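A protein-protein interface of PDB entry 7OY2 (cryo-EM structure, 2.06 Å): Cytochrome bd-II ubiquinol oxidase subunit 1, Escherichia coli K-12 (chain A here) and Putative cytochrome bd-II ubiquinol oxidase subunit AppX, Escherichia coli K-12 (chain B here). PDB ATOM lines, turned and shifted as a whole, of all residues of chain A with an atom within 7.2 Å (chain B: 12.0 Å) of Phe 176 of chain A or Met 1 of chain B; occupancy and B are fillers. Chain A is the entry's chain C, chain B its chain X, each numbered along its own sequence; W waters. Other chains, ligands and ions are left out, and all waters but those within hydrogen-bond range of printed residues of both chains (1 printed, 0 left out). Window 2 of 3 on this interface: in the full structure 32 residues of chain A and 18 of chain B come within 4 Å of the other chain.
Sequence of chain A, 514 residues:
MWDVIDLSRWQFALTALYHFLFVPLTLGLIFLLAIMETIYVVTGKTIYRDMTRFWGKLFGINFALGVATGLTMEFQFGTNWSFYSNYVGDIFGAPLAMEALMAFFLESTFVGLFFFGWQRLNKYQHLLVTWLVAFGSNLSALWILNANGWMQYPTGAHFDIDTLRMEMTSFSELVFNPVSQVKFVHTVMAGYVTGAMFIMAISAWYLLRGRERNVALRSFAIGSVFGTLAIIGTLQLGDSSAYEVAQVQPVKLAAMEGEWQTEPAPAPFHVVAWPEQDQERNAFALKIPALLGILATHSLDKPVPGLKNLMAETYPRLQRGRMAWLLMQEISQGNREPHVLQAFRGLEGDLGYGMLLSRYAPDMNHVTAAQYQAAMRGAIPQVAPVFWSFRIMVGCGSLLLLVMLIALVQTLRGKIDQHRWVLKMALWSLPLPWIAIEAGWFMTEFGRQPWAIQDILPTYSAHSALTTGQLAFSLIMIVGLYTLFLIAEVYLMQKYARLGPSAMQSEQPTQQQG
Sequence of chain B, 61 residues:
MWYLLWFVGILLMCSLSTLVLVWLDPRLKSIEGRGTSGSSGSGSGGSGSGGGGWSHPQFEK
The backbone carbonyl oxygen (O) of Val 175 of chain A lies within hydrogen-bond range of the side-chain hydroxyl (OH) of Tyr 3 of chain B.
The side-chain amide oxygen (OE1) of Gln 181 of chain A sits close to the side-chain sulfur (SD) of Met 1 of chain B.
The backbone NH (N) of Trp 2 of chain B is in hydrogen-bond range of the side-chain amide oxygen (OE1) of Gln 181 of chain A, at 2.7 Å.
O of Leu 174 of chain A sits at hydrogen-bond distance from ND2 of Asn 146 of chain A, at 3.1 Å.
The backbone carbonyl oxygen (O) of Val 175 of chain A is in hydrogen-bond range of the side-chain amide nitrogen (ND2) of Asn 146 of chain A, at 3.4 Å.
The backbone carbonyl oxygen of Asn 146 of chain A is in hydrogen-bond range of the side-chain hydroxyl of Ser 180 of chain A (3.2 Å).
O of Phe 176 of chain A lies within hydrogen-bond range of NE2 of Gln 181 of chain A, at 3.3 Å.
The side-chain amide oxygen (OD1) of Asn 177 of chain A is in hydrogen-bond range of the backbone NH (N) of Ser 180 of chain A (3.5 Å).
The side-chain sulfur of Met 1 of chain B sits close to the backbone NH of Tyr 3 of chain B (3.7 Å).
ND2 of Asn 146 of chain A touches OH of Tyr 3 of chain B, at 3.5 Å.
CD1 of Phe 176 of chain A touches SD of Met 1 of chain B, at 3.6 Å.
C of Ser 180 of chain A touches OH of Tyr 3 of chain B, 3.96 Å away.
CG of Gln 181 of chain A touches OH of Tyr 3 of chain B, 3.4 Å away.
Trp 2 of chain B touches Val 185 of chain A (O to CG2, 3.7 Å).
Trp 6 of chain B touches Val 185 of chain A (CB to CG2, 3.8 Å).
Phe 176 of chain A touches just one residue of chain B: Met 1 (3.6 Å).
Of chain A, only Phe 176 (3.6 Å) and Gln 181 (3.4 Å) come within 4 Å of Met 1 of chain B.
No residue of chain B comes within 4 Å of Ser 172 of chain A.
No residue of chain B comes within 4 Å of Leu 174 of chain A.
Val 175 of chain A touches just one residue of chain B: Tyr 3.
No residue of chain B comes within 4 Å of Asn 177 of chain A.
No residue of chain B comes within 4 Å of Pro 178 of chain A.
Of the printed residues of chain B, Ser 180 of chain A touches Tyr 3.
Of chain B, only Met 1, Trp 2 and Tyr 3 come within 4 Å of Gln 181 of chain A.
Printed residues of chain A within 4 Å of Tyr 3 of chain B: Asn 146 (3.5 Å), Val 175 (2.9 Å), Ser 180 (3.96 Å) and Gln 181 (3.4 Å).
Of the printed residues of chain B, Val 185 of chain A touches Trp 2 (3.7 Å) and Trp 6 (3.8 Å).
The nearest residue of chain A that does not touch Met 1 of chain B is Val 175 of chain A (6.1 Å).
The nearest printed residue of chain A that does not touch Tyr 3 of chain B is Phe 176 of chain A (4.1 Å).
Hydrophobic or aromatic side chains of chain A within 4 Å of the printed part of chain B: Phe 176 and Val 185.
Of the 10 printed residues of chain B, 4 touch a printed residue of chain A.
Hydrophobic or aromatic side chains of chain B that line the printed part of chain A: Met 1, Trp 2, Tyr 3 and Trp 6.
Among the printed residues, no Asp or Glu carboxylate lies within 4 Å of a Lys or Arg side-chain nitrogen of the other chain.
Water W1 lies within hydrogen-bond range of O of Ser 180 of chain A (3.0 Å), OH of Tyr 3 of chain B (3.2 Å) and N of Asn 146 of chain A (3.2 Å).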
ATOM      1  N   TRP A 143      26.867  -4.272  35.535  1.00  0.00           N
ATOM      2  CA  TRP A 143      26.049  -5.478  35.667  1.00  0.00           C
ATOM      3  C   TRP A 143      25.206  -5.473  36.944  1.00  0.00           C
ATOM      4  O   TRP A 143      24.019  -5.822  36.907  1.00  0.00           O
ATOM      5  CB  TRP A 143      26.923  -6.724  35.580  1.00  0.00           C
ATOM      6  CG  TRP A 143      27.461  -6.908  34.203  1.00  0.00           C
ATOM      7  CD1 TRP A 143      28.767  -6.987  33.837  1.00  0.00           C
ATOM      8  CD2 TRP A 143      26.698  -6.988  32.994  1.00  0.00           C
ATOM      9  NE1 TRP A 143      28.869  -7.138  32.476  1.00  0.00           N
ATOM     10  CE2 TRP A 143      27.612  -7.135  31.934  1.00  0.00           C
ATOM     11  CE3 TRP A 143      25.330  -6.960  32.706  1.00  0.00           C
ATOM     12  CZ2 TRP A 143      27.202  -7.254  30.608  1.00  0.00           C
ATOM     13  CZ3 TRP A 143      24.926  -7.068  31.390  1.00  0.00           C
ATOM     14  CH2 TRP A 143      25.860  -7.216  30.356  1.00  0.00           C
ATOM     15  N   ASN A 146      22.516  -3.253  36.362  1.00  0.00           N
ATOM     16  CA  ASN A 146      21.552  -3.902  35.478  1.00  0.00           C
ATOM     17  C   ASN A 146      20.575  -4.754  36.277  1.00  0.00           C
ATOM     18  O   ASN A 146      19.364  -4.709  36.049  1.00  0.00           O
ATOM     19  CB  ASN A 146      22.285  -4.751  34.433  1.00  0.00           C
ATOM     20  CG  ASN A 146      21.403  -5.122  33.245  1.00  0.00           C
ATOM     21  OD1 ASN A 146      21.016  -6.275  33.085  1.00  0.00           O
ATOM     22  ND2 ASN A 146      21.104  -4.146  32.399  1.00  0.00           N
ATOM     23  N   THR A 155      11.845  -6.310  32.836  1.00  0.00           N
ATOM     24  CA  THR A 155      11.617  -6.450  31.406  1.00  0.00           C
ATOM     25  C   THR A 155      12.116  -7.808  30.944  1.00  0.00           C
ATOM     26  O   THR A 155      12.974  -8.426  31.578  1.00  0.00           O
ATOM     27  CB  THR A 155      12.326  -5.351  30.604  1.00  0.00           C
ATOM     28  OG1 THR A 155      13.726  -5.357  30.912  1.00  0.00           O
ATOM     29  CG2 THR A 155      11.750  -3.998  30.936  1.00  0.00           C
ATOM     30  N   PHE A 171      17.046 -11.916  26.551  1.00  0.00           N
ATOM     31  CA  PHE A 171      18.216 -11.405  27.252  1.00  0.00           C
ATOM     32  C   PHE A 171      18.504  -9.958  26.863  1.00  0.00           C
ATOM     33  O   PHE A 171      18.964  -9.165  27.693  1.00  0.00           O
ATOM     34  CB  PHE A 171      19.402 -12.313  26.946  1.00  0.00           C
ATOM     35  CG  PHE A 171      20.666 -11.944  27.639  1.00  0.00           C
ATOM     36  CD1 PHE A 171      20.742 -11.960  29.020  1.00  0.00           C
ATOM     37  CD2 PHE A 171      21.805 -11.659  26.914  1.00  0.00           C
ATOM     38  CE1 PHE A 171      21.913 -11.639  29.666  1.00  0.00           C
ATOM     39  CE2 PHE A 171      22.987 -11.352  27.552  1.00  0.00           C
ATOM     40  CZ  PHE A 171      23.040 -11.341  28.931  1.00  0.00           C
ATOM     41  N   SER A 172      18.228  -9.598  25.608  1.00  0.00           N
ATOM     42  CA  SER A 172      18.504  -8.243  25.142  1.00  0.00           C
ATOM     43  C   SER A 172      17.631  -7.214  25.851  1.00  0.00           C
ATOM     44  O   SER A 172      18.066  -6.082  26.087  1.00  0.00           O
ATOM     45  CB  SER A 172      18.305  -8.160  23.628  1.00  0.00           C
ATOM     46  OG  SER A 172      16.946  -8.354  23.292  1.00  0.00           O
ATOM     47  N   GLU A 173      16.390  -7.576  26.179  1.00  0.00           N
ATOM     48  CA  GLU A 173      15.535  -6.658  26.918  1.00  0.00           C
ATOM     49  C   GLU A 173      16.012  -6.458  28.348  1.00  0.00           C
ATOM     50  O   GLU A 173      15.680  -5.438  28.962  1.00  0.00           O
ATOM     51  CB  GLU A 173      14.088  -7.149  26.906  1.00  0.00           C
ATOM     52  CG  GLU A 173      13.409  -7.051  25.548  1.00  0.00           C
ATOM     53  CD  GLU A 173      11.958  -7.487  25.598  1.00  0.00           C
ATOM     54  OE1 GLU A 173      11.346  -7.376  26.680  1.00  0.00           O
ATOM     55  OE2 GLU A 173      11.439  -7.962  24.564  1.00  0.00           O
ATOM     56  N   LEU A 174      16.771  -7.413  28.886  1.00  0.00           N
ATOM     57  CA  LEU A 174      17.457  -7.220  30.156  1.00  0.00           C
ATOM     58  C   LEU A 174      18.663  -6.305  29.995  1.00  0.00           C
ATOM     59  O   LEU A 174      18.803  -5.312  30.713  1.00  0.00           O
ATOM     60  CB  LEU A 174      17.886  -8.576  30.721  1.00  0.00           C
ATOM     61  CG  LEU A 174      18.956  -8.634  31.811  1.00  0.00           C
ATOM     62  CD1 LEU A 174      18.413  -8.119  33.133  1.00  0.00           C
ATOM     63  CD2 LEU A 174      19.507 -10.046  31.978  1.00  0.00           C
ATOM     64  N   VAL A 175      19.518  -6.614  29.022  1.00  0.00           N
ATOM     65  CA  VAL A 175      20.804  -5.935  28.880  1.00  0.00           C
ATOM     66  C   VAL A 175      20.608  -4.462  28.539  1.00  0.00           C
ATOM     67  O   VAL A 175      21.356  -3.598  29.008  1.00  0.00           O
ATOM     68  CB  VAL A 175      21.663  -6.658  27.827  1.00  0.00           C
ATOM     69  CG1 VAL A 175      22.934  -5.883  27.524  1.00  0.00           C
ATOM     70  CG2 VAL A 175      22.000  -8.055  28.309  1.00  0.00           C
ATOM     71  N   PHE A 176      19.606  -4.150  27.715  1.00  0.00           N
ATOM     72  CA  PHE A 176      19.357  -2.777  27.282  1.00  0.00           C
ATOM     73  C   PHE A 176      18.142  -2.162  27.961  1.00  0.00           C
ATOM     74  O   PHE A 176      17.532  -1.233  27.422  1.00  0.00           O
ATOM     75  CB  PHE A 176      19.217  -2.721  25.763  1.00  0.00           C
ATOM     76  CG  PHE A 176      20.419  -3.237  25.046  1.00  0.00           C
ATOM     77  CD1 PHE A 176      21.641  -2.594  25.174  1.00  0.00           C
ATOM     78  CD2 PHE A 176      20.347  -4.386  24.283  1.00  0.00           C
ATOM     79  CE1 PHE A 176      22.757  -3.076  24.534  1.00  0.00           C
ATOM     80  CE2 PHE A 176      21.463  -4.870  23.637  1.00  0.00           C
ATOM     81  CZ  PHE A 176      22.668  -4.216  23.763  1.00  0.00           C
ATOM     82  N   ASN A 177      17.765  -2.690  29.116  1.00  0.00           N
ATOM     83  CA  ASN A 177      16.788  -2.034  29.969  1.00  0.00           C
ATOM     84  C   ASN A 177      17.143  -0.553  30.103  1.00  0.00           C
ATOM     85  O   ASN A 177      18.228  -0.224  30.598  1.00  0.00           O
ATOM     86  CB  ASN A 177      16.778  -2.722  31.335  1.00  0.00           C
ATOM     87  CG  ASN A 177      15.650  -2.255  32.235  1.00  0.00           C
ATOM     88  OD1 ASN A 177      15.405  -1.064  32.390  1.00  0.00           O
ATOM     89  ND2 ASN A 177      14.963  -3.207  32.848  1.00  0.00           N
ATOM     90  N   PRO A 178      16.274   0.360  29.667  1.00  0.00           N
ATOM     91  CA  PRO A 178      16.623   1.793  29.724  1.00  0.00           C
ATOM     92  C   PRO A 178      16.954   2.286  31.125  1.00  0.00           C
ATOM     93  O   PRO A 178      17.898   3.076  31.312  1.00  0.00           O
ATOM     94  CB  PRO A 178      15.365   2.471  29.165  1.00  0.00           C
ATOM     95  CG  PRO A 178      14.263   1.446  29.300  1.00  0.00           C
ATOM     96  CD  PRO A 178      14.922   0.121  29.143  1.00  0.00           C
ATOM     97  N   VAL A 179      16.207   1.801  32.120  1.00  0.00           N
ATOM     98  CA  VAL A 179      16.468   2.153  33.512  1.00  0.00           C
ATOM     99  C   VAL A 179      17.874   1.739  33.913  1.00  0.00           C
ATOM    100  O   VAL A 179      18.611   2.514  34.523  1.00  0.00           O
ATOM    101  CB  VAL A 179      15.415   1.511  34.431  1.00  0.00           C
ATOM    102  CG1 VAL A 179      15.825   1.656  35.885  1.00  0.00           C
ATOM    103  CG2 VAL A 179      14.074   2.141  34.192  1.00  0.00           C
ATOM    104  N   SER A 180      18.259   0.503  33.595  1.00  0.00           N
ATOM    105  CA  SER A 180      19.590   0.033  33.964  1.00  0.00           C
ATOM    106  C   SER A 180      20.674   0.852  33.275  1.00  0.00           C
ATOM    107  O   SER A 180      21.712   1.141  33.873  1.00  0.00           O
ATOM    108  CB  SER A 180      19.738  -1.448  33.627  1.00  0.00           C
ATOM    109  OG  SER A 180      18.715  -2.209  34.242  1.00  0.00           O
ATOM    110  N   GLN A 181      20.450   1.237  32.019  1.00  0.00           N
ATOM    111  CA  GLN A 181      21.428   2.056  31.309  1.00  0.00           C
ATOM    112  C   GLN A 181      21.672   3.374  32.038  1.00  0.00           C
ATOM    113  O   GLN A 181      22.815   3.711  32.388  1.00  0.00           O
ATOM    114  CB  GLN A 181      20.949   2.320  29.880  1.00  0.00           C
ATOM    115  CG  GLN A 181      20.892   1.094  28.980  1.00  0.00           C
ATOM    116  CD  GLN A 181      20.809   1.461  27.508  1.00  0.00           C
ATOM    117  OE1 GLN A 181      21.244   2.533  27.100  1.00  0.00           O
ATOM    118  NE2 GLN A 181      20.236   0.576  26.710  1.00  0.00           N
ATOM    119  N   VAL A 185      25.078   4.748  34.213  1.00  0.00           N
ATOM    120  CA  VAL A 185      25.900   5.905  33.866  1.00  0.00           C
ATOM    121  C   VAL A 185      25.829   6.955  34.970  1.00  0.00           C
ATOM    122  O   VAL A 185      26.845   7.537  35.361  1.00  0.00           O
ATOM    123  CB  VAL A 185      25.504   6.477  32.492  1.00  0.00           C
ATOM    124  CG1 VAL A 185      26.457   7.588  32.120  1.00  0.00           C
ATOM    125  CG2 VAL A 185      25.571   5.382  31.437  1.00  0.00           C
ATOM    126  N   MET B   1      22.378   4.762  22.800  1.00  0.00           N
ATOM    127  CA  MET B   1      22.590   3.669  23.740  1.00  0.00           C
ATOM    128  C   MET B   1      23.678   4.022  24.758  1.00  0.00           C
ATOM    129  O   MET B   1      24.807   4.355  24.400  1.00  0.00           O
ATOM    130  CB  MET B   1      22.922   2.392  22.976  1.00  0.00           C
ATOM    131  CG  MET B   1      22.365   1.138  23.610  1.00  0.00           C
ATOM    132  SD  MET B   1      23.209   0.646  25.113  1.00  0.00           S
ATOM    133  CE  MET B   1      24.890   0.920  24.593  1.00  0.00           C
ATOM    134  N   TRP B   2      23.316   3.901  26.037  1.00  0.00           N
ATOM    135  CA  TRP B   2      24.043   4.592  27.099  1.00  0.00           C
ATOM    136  C   TRP B   2      25.390   3.955  27.413  1.00  0.00           C
ATOM    137  O   TRP B   2      26.298   4.646  27.873  1.00  0.00           O
ATOM    138  CB  TRP B   2      23.184   4.660  28.356  1.00  0.00           C
ATOM    139  CG  TRP B   2      22.196   5.762  28.302  1.00  0.00           C
ATOM    140  CD1 TRP B   2      20.841   5.651  28.182  1.00  0.00           C
ATOM    141  CD2 TRP B   2      22.483   7.159  28.353  1.00  0.00           C
ATOM    142  NE1 TRP B   2      20.267   6.897  28.169  1.00  0.00           N
ATOM    143  CE2 TRP B   2      21.255   7.841  28.270  1.00  0.00           C
ATOM    144  CE3 TRP B   2      23.661   7.903  28.470  1.00  0.00           C
ATOM    145  CZ2 TRP B   2      21.172   9.229  28.296  1.00  0.00           C
ATOM    146  CZ3 TRP B   2      23.576   9.276  28.491  1.00  0.00           C
ATOM    147  CH2 TRP B   2      22.341   9.927  28.404  1.00  0.00           C
ATOM    148  N   TYR B   3      25.537   2.646  27.222  1.00  0.00           N
ATOM    149  CA  TYR B   3      26.825   2.022  27.519  1.00  0.00           C
ATOM    150  C   TYR B   3      27.904   2.510  26.565  1.00  0.00           C
ATOM    151  O   TYR B   3      29.032   2.798  26.983  1.00  0.00           O
ATOM    152  CB  TYR B   3      26.705   0.501  27.459  1.00  0.00           C
ATOM    153  CG  TYR B   3      25.571  -0.032  28.289  1.00  0.00           C
ATOM    154  CD1 TYR B   3      25.330   0.473  29.556  1.00  0.00           C
ATOM    155  CD2 TYR B   3      24.739  -1.032  27.808  1.00  0.00           C
ATOM    156  CE1 TYR B   3      24.308  -0.004  30.325  1.00  0.00           C
ATOM    157  CE2 TYR B   3      23.704  -1.515  28.572  1.00  0.00           C
ATOM    158  CZ  TYR B   3      23.493  -0.996  29.834  1.00  0.00           C
ATOM    159  OH  TYR B   3      22.468  -1.462  30.612  1.00  0.00           O
ATOM    160  N   LEU B   4      27.571   2.617  25.280  1.00  0.00           N
ATOM    161  CA  LEU B   4      28.510   3.180  24.318  1.00  0.00           C
ATOM    162  C   LEU B   4      28.801   4.638  24.638  1.00  0.00           C
ATOM    163  O   LEU B   4      29.952   5.083  24.542  1.00  0.00           O
ATOM    164  CB  LEU B   4      27.955   3.040  22.901  1.00  0.00           C
ATOM    165  CG  LEU B   4      28.839   3.579  21.775  1.00  0.00           C
ATOM    166  CD1 LEU B   4      30.265   3.069  21.904  1.00  0.00           C
ATOM    167  CD2 LEU B   4      28.264   3.210  20.420  1.00  0.00           C
ATOM    168  N   LEU B   5      27.766   5.399  25.002  1.00  0.00           N
ATOM    169  CA  LEU B   5      27.976   6.794  25.357  1.00  0.00           C
ATOM    170  C   LEU B   5      28.892   6.908  26.560  1.00  0.00           C
ATOM    171  O   LEU B   5      29.771   7.765  26.591  1.00  0.00           O
ATOM    172  CB  LEU B   5      26.652   7.490  25.647  1.00  0.00           C
ATOM    173  CG  LEU B   5      25.669   7.728  24.501  1.00  0.00           C
ATOM    174  CD1 LEU B   5      24.484   8.523  25.021  1.00  0.00           C
ATOM    175  CD2 LEU B   5      26.339   8.445  23.354  1.00  0.00           C
ATOM    176  N   TRP B   6      28.700   6.044  27.556  1.00  0.00           N
ATOM    177  CA  TRP B   6      29.552   6.060  28.736  1.00  0.00           C
ATOM    178  C   TRP B   6      30.988   5.718  28.374  1.00  0.00           C
ATOM    179  O   TRP B   6      31.925   6.336  28.880  1.00  0.00           O
ATOM    180  CB  TRP B   6      29.035   5.082  29.788  1.00  0.00           C
ATOM    181  CG  TRP B   6      30.083   4.798  30.800  1.00  0.00           C
ATOM    182  CD1 TRP B   6      30.415   5.573  31.871  1.00  0.00           C
ATOM    183  CD2 TRP B   6      30.988   3.696  30.805  1.00  0.00           C
ATOM    184  NE1 TRP B   6      31.456   5.008  32.556  1.00  0.00           N
ATOM    185  CE2 TRP B   6      31.827   3.853  31.923  1.00  0.00           C
ATOM    186  CE3 TRP B   6      31.165   2.581  29.980  1.00  0.00           C
ATOM    187  CZ2 TRP B   6      32.820   2.938  32.241  1.00  0.00           C
ATOM    188  CZ3 TRP B   6      32.157   1.673  30.298  1.00  0.00           C
ATOM    189  CH2 TRP B   6      32.970   1.858  31.418  1.00  0.00           C
ATOM    190  N   PHE B   7      31.182   4.706  27.531  1.00  0.00           N
ATOM    191  CA  PHE B   7      32.533   4.311  27.144  1.00  0.00           C
ATOM    192  C   PHE B   7      33.251   5.456  26.434  1.00  0.00           C
ATOM    193  O   PHE B   7      34.364   5.855  26.820  1.00  0.00           O
ATOM    194  CB  PHE B   7      32.460   3.073  26.252  1.00  0.00           C
ATOM    195  CG  PHE B   7      33.773   2.400  26.031  1.00  0.00           C
ATOM    196  CD1 PHE B   7      34.389   1.704  27.050  1.00  0.00           C
ATOM    197  CD2 PHE B   7      34.381   2.440  24.791  1.00  0.00           C
ATOM    198  CE1 PHE B   7      35.593   1.071  26.841  1.00  0.00           C
ATOM    199  CE2 PHE B   7      35.588   1.809  24.579  1.00  0.00           C
ATOM    200  CZ  PHE B   7      36.195   1.126  25.602  1.00  0.00           C
ATOM    201  N   VAL B   8      32.599   6.029  25.422  1.00  0.00           N
ATOM    202  CA  VAL B   8      33.169   7.173  24.716  1.00  0.00           C
ATOM    203  C   VAL B   8      33.401   8.328  25.682  1.00  0.00           C
ATOM    204  O   VAL B   8      34.456   8.967  25.661  1.00  0.00           O
ATOM    205  CB  VAL B   8      32.258   7.592  23.545  1.00  0.00           C
ATOM    206  CG1 VAL B   8      32.841   8.806  22.816  1.00  0.00           C
ATOM    207  CG2 VAL B   8      32.043   6.436  22.588  1.00  0.00           C
ATOM    208  N   GLY B   9      32.426   8.601  26.551  1.00  0.00           N
ATOM    209  CA  GLY B   9      32.507   9.758  27.419  1.00  0.00           C
ATOM    210  C   GLY B   9      33.586   9.645  28.474  1.00  0.00           C
ATOM    211  O   GLY B   9      34.231  10.632  28.811  1.00  0.00           O
ATOM    212  N   ILE B  10      33.785   8.447  29.027  1.00  0.00           N
ATOM    213  CA  ILE B  10      34.851   8.272  30.007  1.00  0.00           C
ATOM    214  C   ILE B  10      36.208   8.350  29.323  1.00  0.00           C
ATOM    215  O   ILE B  10      37.164   8.911  29.881  1.00  0.00           O
ATOM    216  CB  ILE B  10      34.664   6.962  30.805  1.00  0.00           C
ATOM    217  CG1 ILE B  10      35.638   6.906  31.988  1.00  0.00           C
ATOM    218  CG2 ILE B  10      34.827   5.736  29.929  1.00  0.00           C
ATOM    219  CD1 ILE B  10      35.472   8.047  32.992  1.00  0.00           C
HETATM  220  O   HOH W   1      23.146  -1.522  33.695  1.00  0.00           O
